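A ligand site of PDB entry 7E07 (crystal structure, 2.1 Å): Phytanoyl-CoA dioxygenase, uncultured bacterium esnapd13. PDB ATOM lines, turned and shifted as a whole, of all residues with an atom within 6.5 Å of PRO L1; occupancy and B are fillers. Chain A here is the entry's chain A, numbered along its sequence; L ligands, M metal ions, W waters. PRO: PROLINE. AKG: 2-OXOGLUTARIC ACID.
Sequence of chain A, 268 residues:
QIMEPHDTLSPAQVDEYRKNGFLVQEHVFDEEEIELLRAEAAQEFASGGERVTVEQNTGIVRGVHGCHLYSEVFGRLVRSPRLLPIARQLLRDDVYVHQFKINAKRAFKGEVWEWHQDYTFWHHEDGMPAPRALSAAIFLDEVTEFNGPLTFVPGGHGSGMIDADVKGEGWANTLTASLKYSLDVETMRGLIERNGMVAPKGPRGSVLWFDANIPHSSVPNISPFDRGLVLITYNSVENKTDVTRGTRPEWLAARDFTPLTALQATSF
NH1 of Arg 248 is in hydrogen-bond range of OG1 of Thr 174. O of Trp 171 sits at hydrogen-bond distance from OG1 of Thr 174 (2.6 Å). NH2 of Arg 248 lies within salt-bridge range of OD2 of Asp 126 (3.0 Å). NE2 of Gln 99 sits close to NE1 of Trp 122 (3.5 Å). The side-chain amide nitrogen (NE2) of Gln 99 lies within hydrogen-bond range of the backbone carbonyl oxygen (O) of Leu 252, at 2.9 Å. NZ of Lys 101 is in hydrogen-bond range of OE1 of Gln 99 (2.6 Å).
The guanidinium group (NH1) of Arg 248 is in salt-bridge range of an oxygen (OXT) of PRO L1, 2.7 Å away. An oxygen (O) of PRO L1 lies within hydrogen-bond range of the side-chain amide nitrogen (NE2) of Gln 99, 2.8 Å away. O of Thr 174 lies within hydrogen-bond range of N of PRO L1 (2.9 Å). The indole nitrogen of Trp 122 sits at hydrogen-bond distance from an oxygen (O) of PRO L1 (3.0 Å).
Water W1 lies within hydrogen-bond range of N of PRO L1 (2.7 Å) and O2 of AKG L2 (2.8 Å).
CD2 of His 116 touches CG of PRO L1, at 3.7 Å. Asp 118 touches PRO L1. Phe 121 touches PRO L1. Hydrophobic or aromatic side chains that line PRO L1: His 116, Phe 121 and Trp 122. Within 4 Å of PRO L1: Gln 99, His 116, Asp 118, Phe 121, Trp 122, Thr 174 and Arg 248.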
ATOM      1  N   HIS A  98      -5.486  13.567 -21.688  1.00  0.00           N
ATOM      2  CA  HIS A  98      -4.099  13.603 -22.174  1.00  0.00           C
ATOM      3  C   HIS A  98      -4.058  13.262 -23.629  1.00  0.00           C
ATOM      4  O   HIS A  98      -3.363  13.939 -24.400  1.00  0.00           O
ATOM      5  CB  HIS A  98      -3.239  12.643 -21.434  1.00  0.00           C
ATOM      6  CG  HIS A  98      -1.870  12.513 -21.992  1.00  0.00           C
ATOM      7  ND1 HIS A  98      -0.963  13.548 -21.976  1.00  0.00           N
ATOM      8  CD2 HIS A  98      -1.253  11.465 -22.598  1.00  0.00           C
ATOM      9  CE1 HIS A  98       0.156  13.159 -22.583  1.00  0.00           C
ATOM     10  NE2 HIS A  98       0.017  11.903 -22.959  1.00  0.00           N
ATOM     11  N   GLN A  99      -4.864  12.243 -24.037  1.00  0.00           N
ATOM     12  CA  GLN A  99      -4.855  11.804 -25.425  1.00  0.00           C
ATOM     13  C   GLN A  99      -6.163  11.188 -25.770  1.00  0.00           C
ATOM     14  O   GLN A  99      -6.865  10.620 -24.911  1.00  0.00           O
ATOM     15  CB  GLN A  99      -3.697  10.762 -25.578  1.00  0.00           C
ATOM     16  CG  GLN A  99      -3.479  10.109 -26.912  1.00  0.00           C
ATOM     17  CD  GLN A  99      -2.253   9.193 -26.883  1.00  0.00           C
ATOM     18  OE1 GLN A  99      -2.384   7.978 -26.820  1.00  0.00           O
ATOM     19  NE2 GLN A  99      -1.060   9.774 -26.910  1.00  0.00           N
ATOM     20  N   LYS A 101      -7.712   8.924 -29.104  1.00  0.00           N
ATOM     21  CA  LYS A 101      -7.527   8.317 -30.441  1.00  0.00           C
ATOM     22  C   LYS A 101      -8.590   7.309 -30.777  1.00  0.00           C
ATOM     23  O   LYS A 101      -9.233   6.707 -29.887  1.00  0.00           O
ATOM     24  CB  LYS A 101      -6.097   7.745 -30.565  1.00  0.00           C
ATOM     25  CG  LYS A 101      -5.867   6.534 -29.664  1.00  0.00           C
ATOM     26  CD  LYS A 101      -4.382   6.246 -29.392  1.00  0.00           C
ATOM     27  CE  LYS A 101      -4.185   5.328 -28.186  1.00  0.00           C
ATOM     28  NZ  LYS A 101      -4.111   6.048 -26.847  1.00  0.00           N
ATOM     29  N   TRP A 113      -0.161  -4.862 -33.082  1.00  0.00           N
ATOM     30  CA  TRP A 113       0.460  -3.899 -32.121  1.00  0.00           C
ATOM     31  C   TRP A 113       1.296  -4.654 -31.120  1.00  0.00           C
ATOM     32  O   TRP A 113       0.777  -5.436 -30.352  1.00  0.00           O
ATOM     33  CB  TRP A 113      -0.597  -3.089 -31.389  1.00  0.00           C
ATOM     34  CG  TRP A 113      -1.367  -2.108 -32.232  1.00  0.00           C
ATOM     35  CD1 TRP A 113      -2.357  -2.421 -33.126  1.00  0.00           C
ATOM     36  CD2 TRP A 113      -1.233  -0.673 -32.275  1.00  0.00           C
ATOM     37  NE1 TRP A 113      -2.842  -1.263 -33.735  1.00  0.00           N
ATOM     38  CE2 TRP A 113      -2.181  -0.183 -33.222  1.00  0.00           C
ATOM     39  CE3 TRP A 113      -0.414   0.253 -31.616  1.00  0.00           C
ATOM     40  CZ2 TRP A 113      -2.320   1.204 -33.505  1.00  0.00           C
ATOM     41  CZ3 TRP A 113      -0.526   1.636 -31.949  1.00  0.00           C
ATOM     42  CH2 TRP A 113      -1.478   2.081 -32.875  1.00  0.00           C
ATOM     43  N   HIS A 116       3.403  -3.449 -25.206  1.00  0.00           N
ATOM     44  CA  HIS A 116       3.832  -2.137 -24.734  1.00  0.00           C
ATOM     45  C   HIS A 116       2.999  -1.671 -23.544  1.00  0.00           C
ATOM     46  O   HIS A 116       1.939  -2.259 -23.184  1.00  0.00           O
ATOM     47  CB  HIS A 116       3.829  -1.094 -25.855  1.00  0.00           C
ATOM     48  CG  HIS A 116       2.473  -0.674 -26.296  1.00  0.00           C
ATOM     49  ND1 HIS A 116       1.711  -1.416 -27.164  1.00  0.00           N
ATOM     50  CD2 HIS A 116       1.723   0.409 -25.964  1.00  0.00           C
ATOM     51  CE1 HIS A 116       0.543  -0.828 -27.337  1.00  0.00           C
ATOM     52  NE2 HIS A 116       0.535   0.286 -26.631  1.00  0.00           N
ATOM     53  N   GLN A 117       3.585  -0.702 -22.834  1.00  0.00           N
ATOM     54  CA  GLN A 117       2.939   0.003 -21.742  1.00  0.00           C
ATOM     55  C   GLN A 117       2.741   1.420 -22.250  1.00  0.00           C
ATOM     56  O   GLN A 117       3.694   2.040 -22.794  1.00  0.00           O
ATOM     57  CB  GLN A 117       3.781  -0.031 -20.505  1.00  0.00           C
ATOM     58  CG  GLN A 117       3.835  -1.377 -19.896  1.00  0.00           C
ATOM     59  CD  GLN A 117       4.907  -1.445 -18.809  1.00  0.00           C
ATOM     60  OE1 GLN A 117       6.085  -1.275 -19.121  1.00  0.00           O
ATOM     61  NE2 GLN A 117       4.524  -1.693 -17.552  1.00  0.00           N
ATOM     62  N   ASP A 118       1.517   1.929 -22.201  1.00  0.00           N
ATOM     63  CA  ASP A 118       1.264   3.293 -22.737  1.00  0.00           C
ATOM     64  C   ASP A 118       2.083   4.349 -21.991  1.00  0.00           C
ATOM     65  O   ASP A 118       2.499   5.312 -22.557  1.00  0.00           O
ATOM     66  CB  ASP A 118      -0.200   3.706 -22.602  1.00  0.00           C
ATOM     67  CG  ASP A 118      -1.138   2.954 -23.546  1.00  0.00           C
ATOM     68  OD1 ASP A 118      -0.677   2.357 -24.560  1.00  0.00           O
ATOM     69  OD2 ASP A 118      -2.355   2.958 -23.228  1.00  0.00           O
ATOM     70  N   TYR A 119       2.245   4.153 -20.696  1.00  0.00           N
ATOM     71  CA  TYR A 119       2.857   5.176 -19.821  1.00  0.00           C
ATOM     72  C   TYR A 119       4.337   5.370 -20.217  1.00  0.00           C
ATOM     73  O   TYR A 119       4.921   6.427 -19.976  1.00  0.00           O
ATOM     74  CB  TYR A 119       2.784   4.743 -18.388  1.00  0.00           C
ATOM     75  CG  TYR A 119       3.580   5.608 -17.418  1.00  0.00           C
ATOM     76  CD1 TYR A 119       3.292   6.971 -17.263  1.00  0.00           C
ATOM     77  CD2 TYR A 119       4.674   5.085 -16.701  1.00  0.00           C
ATOM     78  CE1 TYR A 119       4.048   7.767 -16.397  1.00  0.00           C
ATOM     79  CE2 TYR A 119       5.433   5.893 -15.857  1.00  0.00           C
ATOM     80  CZ  TYR A 119       5.093   7.234 -15.687  1.00  0.00           C
ATOM     81  OH  TYR A 119       5.812   8.070 -14.861  1.00  0.00           O
ATOM     82  N   PHE A 121       5.544   5.672 -23.161  1.00  0.00           N
ATOM     83  CA  PHE A 121       5.565   6.752 -24.107  1.00  0.00           C
ATOM     84  C   PHE A 121       5.209   8.125 -23.474  1.00  0.00           C
ATOM     85  O   PHE A 121       5.738   9.146 -23.829  1.00  0.00           O
ATOM     86  CB  PHE A 121       4.522   6.495 -25.215  1.00  0.00           C
ATOM     87  CG  PHE A 121       4.780   5.272 -26.017  1.00  0.00           C
ATOM     88  CD1 PHE A 121       4.681   3.981 -25.433  1.00  0.00           C
ATOM     89  CD2 PHE A 121       5.154   5.369 -27.360  1.00  0.00           C
ATOM     90  CE1 PHE A 121       4.948   2.844 -26.166  1.00  0.00           C
ATOM     91  CE2 PHE A 121       5.421   4.208 -28.096  1.00  0.00           C
ATOM     92  CZ  PHE A 121       5.307   2.948 -27.498  1.00  0.00           C
ATOM     93  N   TRP A 122       4.218   8.132 -22.575  1.00  0.00           N
ATOM     94  CA  TRP A 122       3.693   9.364 -22.057  1.00  0.00           C
ATOM     95  C   TRP A 122       4.760   9.936 -21.099  1.00  0.00           C
ATOM     96  O   TRP A 122       5.030  11.105 -21.141  1.00  0.00           O
ATOM     97  CB  TRP A 122       2.356   9.123 -21.364  1.00  0.00           C
ATOM     98  CG  TRP A 122       1.332   8.593 -22.251  1.00  0.00           C
ATOM     99  CD1 TRP A 122       1.214   8.824 -23.558  1.00  0.00           C
ATOM    100  CD2 TRP A 122       0.216   7.808 -21.872  1.00  0.00           C
ATOM    101  NE1 TRP A 122       0.086   8.218 -24.039  1.00  0.00           N
ATOM    102  CE2 TRP A 122      -0.531   7.559 -23.009  1.00  0.00           C
ATOM    103  CE3 TRP A 122      -0.247   7.314 -20.653  1.00  0.00           C
ATOM    104  CZ2 TRP A 122      -1.784   6.871 -22.983  1.00  0.00           C
ATOM    105  CZ3 TRP A 122      -1.436   6.549 -20.639  1.00  0.00           C
ATOM    106  CH2 TRP A 122      -2.164   6.315 -21.813  1.00  0.00           C
ATOM    107  N   GLU A 125       8.093  10.689 -23.789  1.00  0.00           N
ATOM    108  CA  GLU A 125       7.818  11.646 -24.855  1.00  0.00           C
ATOM    109  C   GLU A 125       7.134  12.922 -24.366  1.00  0.00           C
ATOM    110  O   GLU A 125       7.266  13.998 -24.976  1.00  0.00           O
ATOM    111  CB  GLU A 125       6.903  11.001 -25.920  1.00  0.00           C
ATOM    112  CG  GLU A 125       7.408   9.732 -26.588  1.00  0.00           C
ATOM    113  CD  GLU A 125       8.564   9.998 -27.564  1.00  0.00           C
ATOM    114  OE1 GLU A 125       8.340  10.710 -28.578  1.00  0.00           O
ATOM    115  OE2 GLU A 125       9.686   9.478 -27.279  1.00  0.00           O
ATOM    116  N   ASP A 126       6.335  12.777 -23.311  1.00  0.00           N
ATOM    117  CA  ASP A 126       5.380  13.851 -22.987  1.00  0.00           C
ATOM    118  C   ASP A 126       5.612  14.486 -21.615  1.00  0.00           C
ATOM    119  O   ASP A 126       5.041  15.507 -21.362  1.00  0.00           O
ATOM    120  CB  ASP A 126       3.929  13.322 -23.058  1.00  0.00           C
ATOM    121  CG  ASP A 126       3.543  12.803 -24.422  1.00  0.00           C
ATOM    122  OD1 ASP A 126       4.043  13.299 -25.465  1.00  0.00           O
ATOM    123  OD2 ASP A 126       2.633  11.946 -24.438  1.00  0.00           O
ATOM    124  N   TRP A 171       9.047  11.068 -33.003  1.00  0.00           N
ATOM    125  CA  TRP A 171       7.783  10.443 -32.543  1.00  0.00           C
ATOM    126  C   TRP A 171       6.918   9.754 -33.621  1.00  0.00           C
ATOM    127  O   TRP A 171       5.938   9.155 -33.271  1.00  0.00           O
ATOM    128  CB  TRP A 171       6.910  11.475 -31.757  1.00  0.00           C
ATOM    129  CG  TRP A 171       6.544  12.765 -32.513  1.00  0.00           C
ATOM    130  CD1 TRP A 171       7.164  13.983 -32.370  1.00  0.00           C
ATOM    131  CD2 TRP A 171       5.452  12.994 -33.450  1.00  0.00           C
ATOM    132  NE1 TRP A 171       6.536  14.940 -33.148  1.00  0.00           N
ATOM    133  CE2 TRP A 171       5.519  14.362 -33.854  1.00  0.00           C
ATOM    134  CE3 TRP A 171       4.471  12.163 -34.030  1.00  0.00           C
ATOM    135  CZ2 TRP A 171       4.656  14.908 -34.788  1.00  0.00           C
ATOM    136  CZ3 TRP A 171       3.597  12.721 -34.986  1.00  0.00           C
ATOM    137  CH2 TRP A 171       3.687  14.083 -35.353  1.00  0.00           C
ATOM    138  N   THR A 174       5.833   6.244 -32.685  1.00  0.00           N
ATOM    139  CA  THR A 174       4.950   6.042 -31.531  1.00  0.00           C
ATOM    140  C   THR A 174       3.527   5.637 -31.943  1.00  0.00           C
ATOM    141  O   THR A 174       2.811   5.060 -31.151  1.00  0.00           O
ATOM    142  CB  THR A 174       4.901   7.291 -30.618  1.00  0.00           C
ATOM    143  OG1 THR A 174       4.362   8.429 -31.326  1.00  0.00           O
ATOM    144  CG2 THR A 174       6.277   7.580 -30.061  1.00  0.00           C
ATOM    145  N   LEU A 175       3.134   5.942 -33.187  1.00  0.00           N
ATOM    146  CA  LEU A 175       1.778   5.592 -33.681  1.00  0.00           C
ATOM    147  C   LEU A 175       1.757   4.344 -34.602  1.00  0.00           C
ATOM    148  O   LEU A 175       0.683   3.927 -35.028  1.00  0.00           O
ATOM    149  CB  LEU A 175       1.191   6.816 -34.380  1.00  0.00           C
ATOM    150  CG  LEU A 175       1.301   8.120 -33.604  1.00  0.00           C
ATOM    151  CD1 LEU A 175       0.725   9.250 -34.429  1.00  0.00           C
ATOM    152  CD2 LEU A 175       0.604   8.002 -32.244  1.00  0.00           C
ATOM    153  N   THR A 176       2.925   3.745 -34.873  1.00  0.00           N
ATOM    154  CA  THR A 176       3.072   2.719 -35.908  1.00  0.00           C
ATOM    155  C   THR A 176       3.058   1.278 -35.298  1.00  0.00           C
ATOM    156  O   THR A 176       3.347   1.099 -34.110  1.00  0.00           O
ATOM    157  CB  THR A 176       4.306   2.958 -36.831  1.00  0.00           C
ATOM    158  OG1 THR A 176       5.509   2.997 -36.059  1.00  0.00           O
ATOM    159  CG2 THR A 176       4.200   4.284 -37.610  1.00  0.00           C
ATOM    160  N   LEU A 179       6.532  -0.290 -32.812  1.00  0.00           N
ATOM    161  CA  LEU A 179       6.494   0.820 -31.839  1.00  0.00           C
ATOM    162  C   LEU A 179       7.874   1.232 -31.419  1.00  0.00           C
ATOM    163  O   LEU A 179       8.779   0.409 -31.364  1.00  0.00           O
ATOM    164  CB  LEU A 179       5.708   0.417 -30.578  1.00  0.00           C
ATOM    165  CG  LEU A 179       4.199   0.302 -30.792  1.00  0.00           C
ATOM    166  CD1 LEU A 179       3.552  -0.468 -29.648  1.00  0.00           C
ATOM    167  CD2 LEU A 179       3.592   1.704 -30.956  1.00  0.00           C
ATOM    168  N   HIS A 216       0.072  -4.295 -22.874  1.00  0.00           N
ATOM    169  CA  HIS A 216      -0.967  -4.834 -23.758  1.00  0.00           C
ATOM    170  C   HIS A 216      -0.500  -4.981 -25.155  1.00  0.00           C
ATOM    171  O   HIS A 216       0.483  -4.325 -25.642  1.00  0.00           O
ATOM    172  CB  HIS A 216      -2.302  -3.996 -23.714  1.00  0.00           C
ATOM    173  CG  HIS A 216      -2.112  -2.521 -23.990  1.00  0.00           C
ATOM    174  ND1 HIS A 216      -1.590  -1.677 -23.061  1.00  0.00           N
ATOM    175  CD2 HIS A 216      -2.332  -1.774 -25.092  1.00  0.00           C
ATOM    176  CE1 HIS A 216      -1.530  -0.456 -23.567  1.00  0.00           C
ATOM    177  NE2 HIS A 216      -1.910  -0.502 -24.822  1.00  0.00           N
ATOM    178  N   ARG A 248       5.789  16.475 -28.555  1.00  0.00           N
ATOM    179  CA  ARG A 248       4.758  16.090 -29.536  1.00  0.00           C
ATOM    180  C   ARG A 248       3.657  17.087 -29.585  1.00  0.00           C
ATOM    181  O   ARG A 248       3.499  17.892 -28.689  1.00  0.00           O
ATOM    182  CB  ARG A 248       4.181  14.744 -29.148  1.00  0.00           C
ATOM    183  CG  ARG A 248       5.245  13.664 -29.047  1.00  0.00           C
ATOM    184  CD  ARG A 248       4.650  12.273 -29.198  1.00  0.00           C
ATOM    185  NE  ARG A 248       3.889  11.829 -28.042  1.00  0.00           N
ATOM    186  CZ  ARG A 248       3.306  10.633 -27.947  1.00  0.00           C
ATOM    187  NH1 ARG A 248       3.451   9.739 -28.935  1.00  0.00           N
ATOM    188  NH2 ARG A 248       2.621  10.265 -26.875  1.00  0.00           N
ATOM    189  N   LEU A 252      -1.639  14.927 -29.826  1.00  0.00           N
ATOM    190  CA  LEU A 252      -1.170  13.694 -29.213  1.00  0.00           C
ATOM    191  C   LEU A 252      -0.988  13.758 -27.719  1.00  0.00           C
ATOM    192  O   LEU A 252      -0.995  12.694 -27.016  1.00  0.00           O
ATOM    193  CB  LEU A 252       0.207  13.268 -29.785  1.00  0.00           C
ATOM    194  CG  LEU A 252       0.191  12.651 -31.176  1.00  0.00           C
ATOM    195  CD1 LEU A 252       1.580  12.403 -31.745  1.00  0.00           C
ATOM    196  CD2 LEU A 252      -0.618  11.337 -31.180  1.00  0.00           C
HETATM  197  N   PRO L   1       0.923   5.016 -28.992  1.00  0.00           N
HETATM  198  CA  PRO L   1       0.377   5.965 -27.976  1.00  0.00           C
HETATM  199  C   PRO L   1       1.299   7.170 -27.788  1.00  0.00           C
HETATM  200  O   PRO L   1       1.102   7.952 -26.877  1.00  0.00           O
HETATM  201  CB  PRO L   1       0.326   5.135 -26.696  1.00  0.00           C
HETATM  202  CG  PRO L   1       1.284   3.981 -26.932  1.00  0.00           C
HETATM  203  CD  PRO L   1       1.235   3.696 -28.401  1.00  0.00           C
HETATM  204  OXT PRO L   1       2.256   7.372 -28.532  1.00  0.00           O
HETATM  205  C1  AKG L   2      -2.441   2.089 -28.424  1.00  0.00           C
HETATM  206  O1  AKG L   2      -1.645   2.502 -27.495  1.00  0.00           O
HETATM  207  O2  AKG L   2      -2.772   2.774 -29.443  1.00  0.00           O
HETATM  208  C2  AKG L   2      -2.975   0.714 -28.301  1.00  0.00           C
HETATM  209  O5  AKG L   2      -2.525  -0.015 -27.469  1.00  0.00           O
HETATM  210  C3  AKG L   2      -4.186   0.226 -29.037  1.00  0.00           C
HETATM  211  C4  AKG L   2      -3.957  -0.932 -30.008  1.00  0.00           C
HETATM  212  C5  AKG L   2      -5.245  -1.450 -30.635  1.00  0.00           C
HETATM  213  O3  AKG L   2      -5.426  -2.698 -30.767  1.00  0.00           O
HETATM  214  O4  AKG L   2      -6.124  -0.624 -31.052  1.00  0.00           O
HETATM  215 FE    FE M   1      -1.504   1.164 -26.084  1.00  0.00          FE
HETATM  216  O   HOH W   1      -1.340   5.020 -30.387  1.00  0.00           O
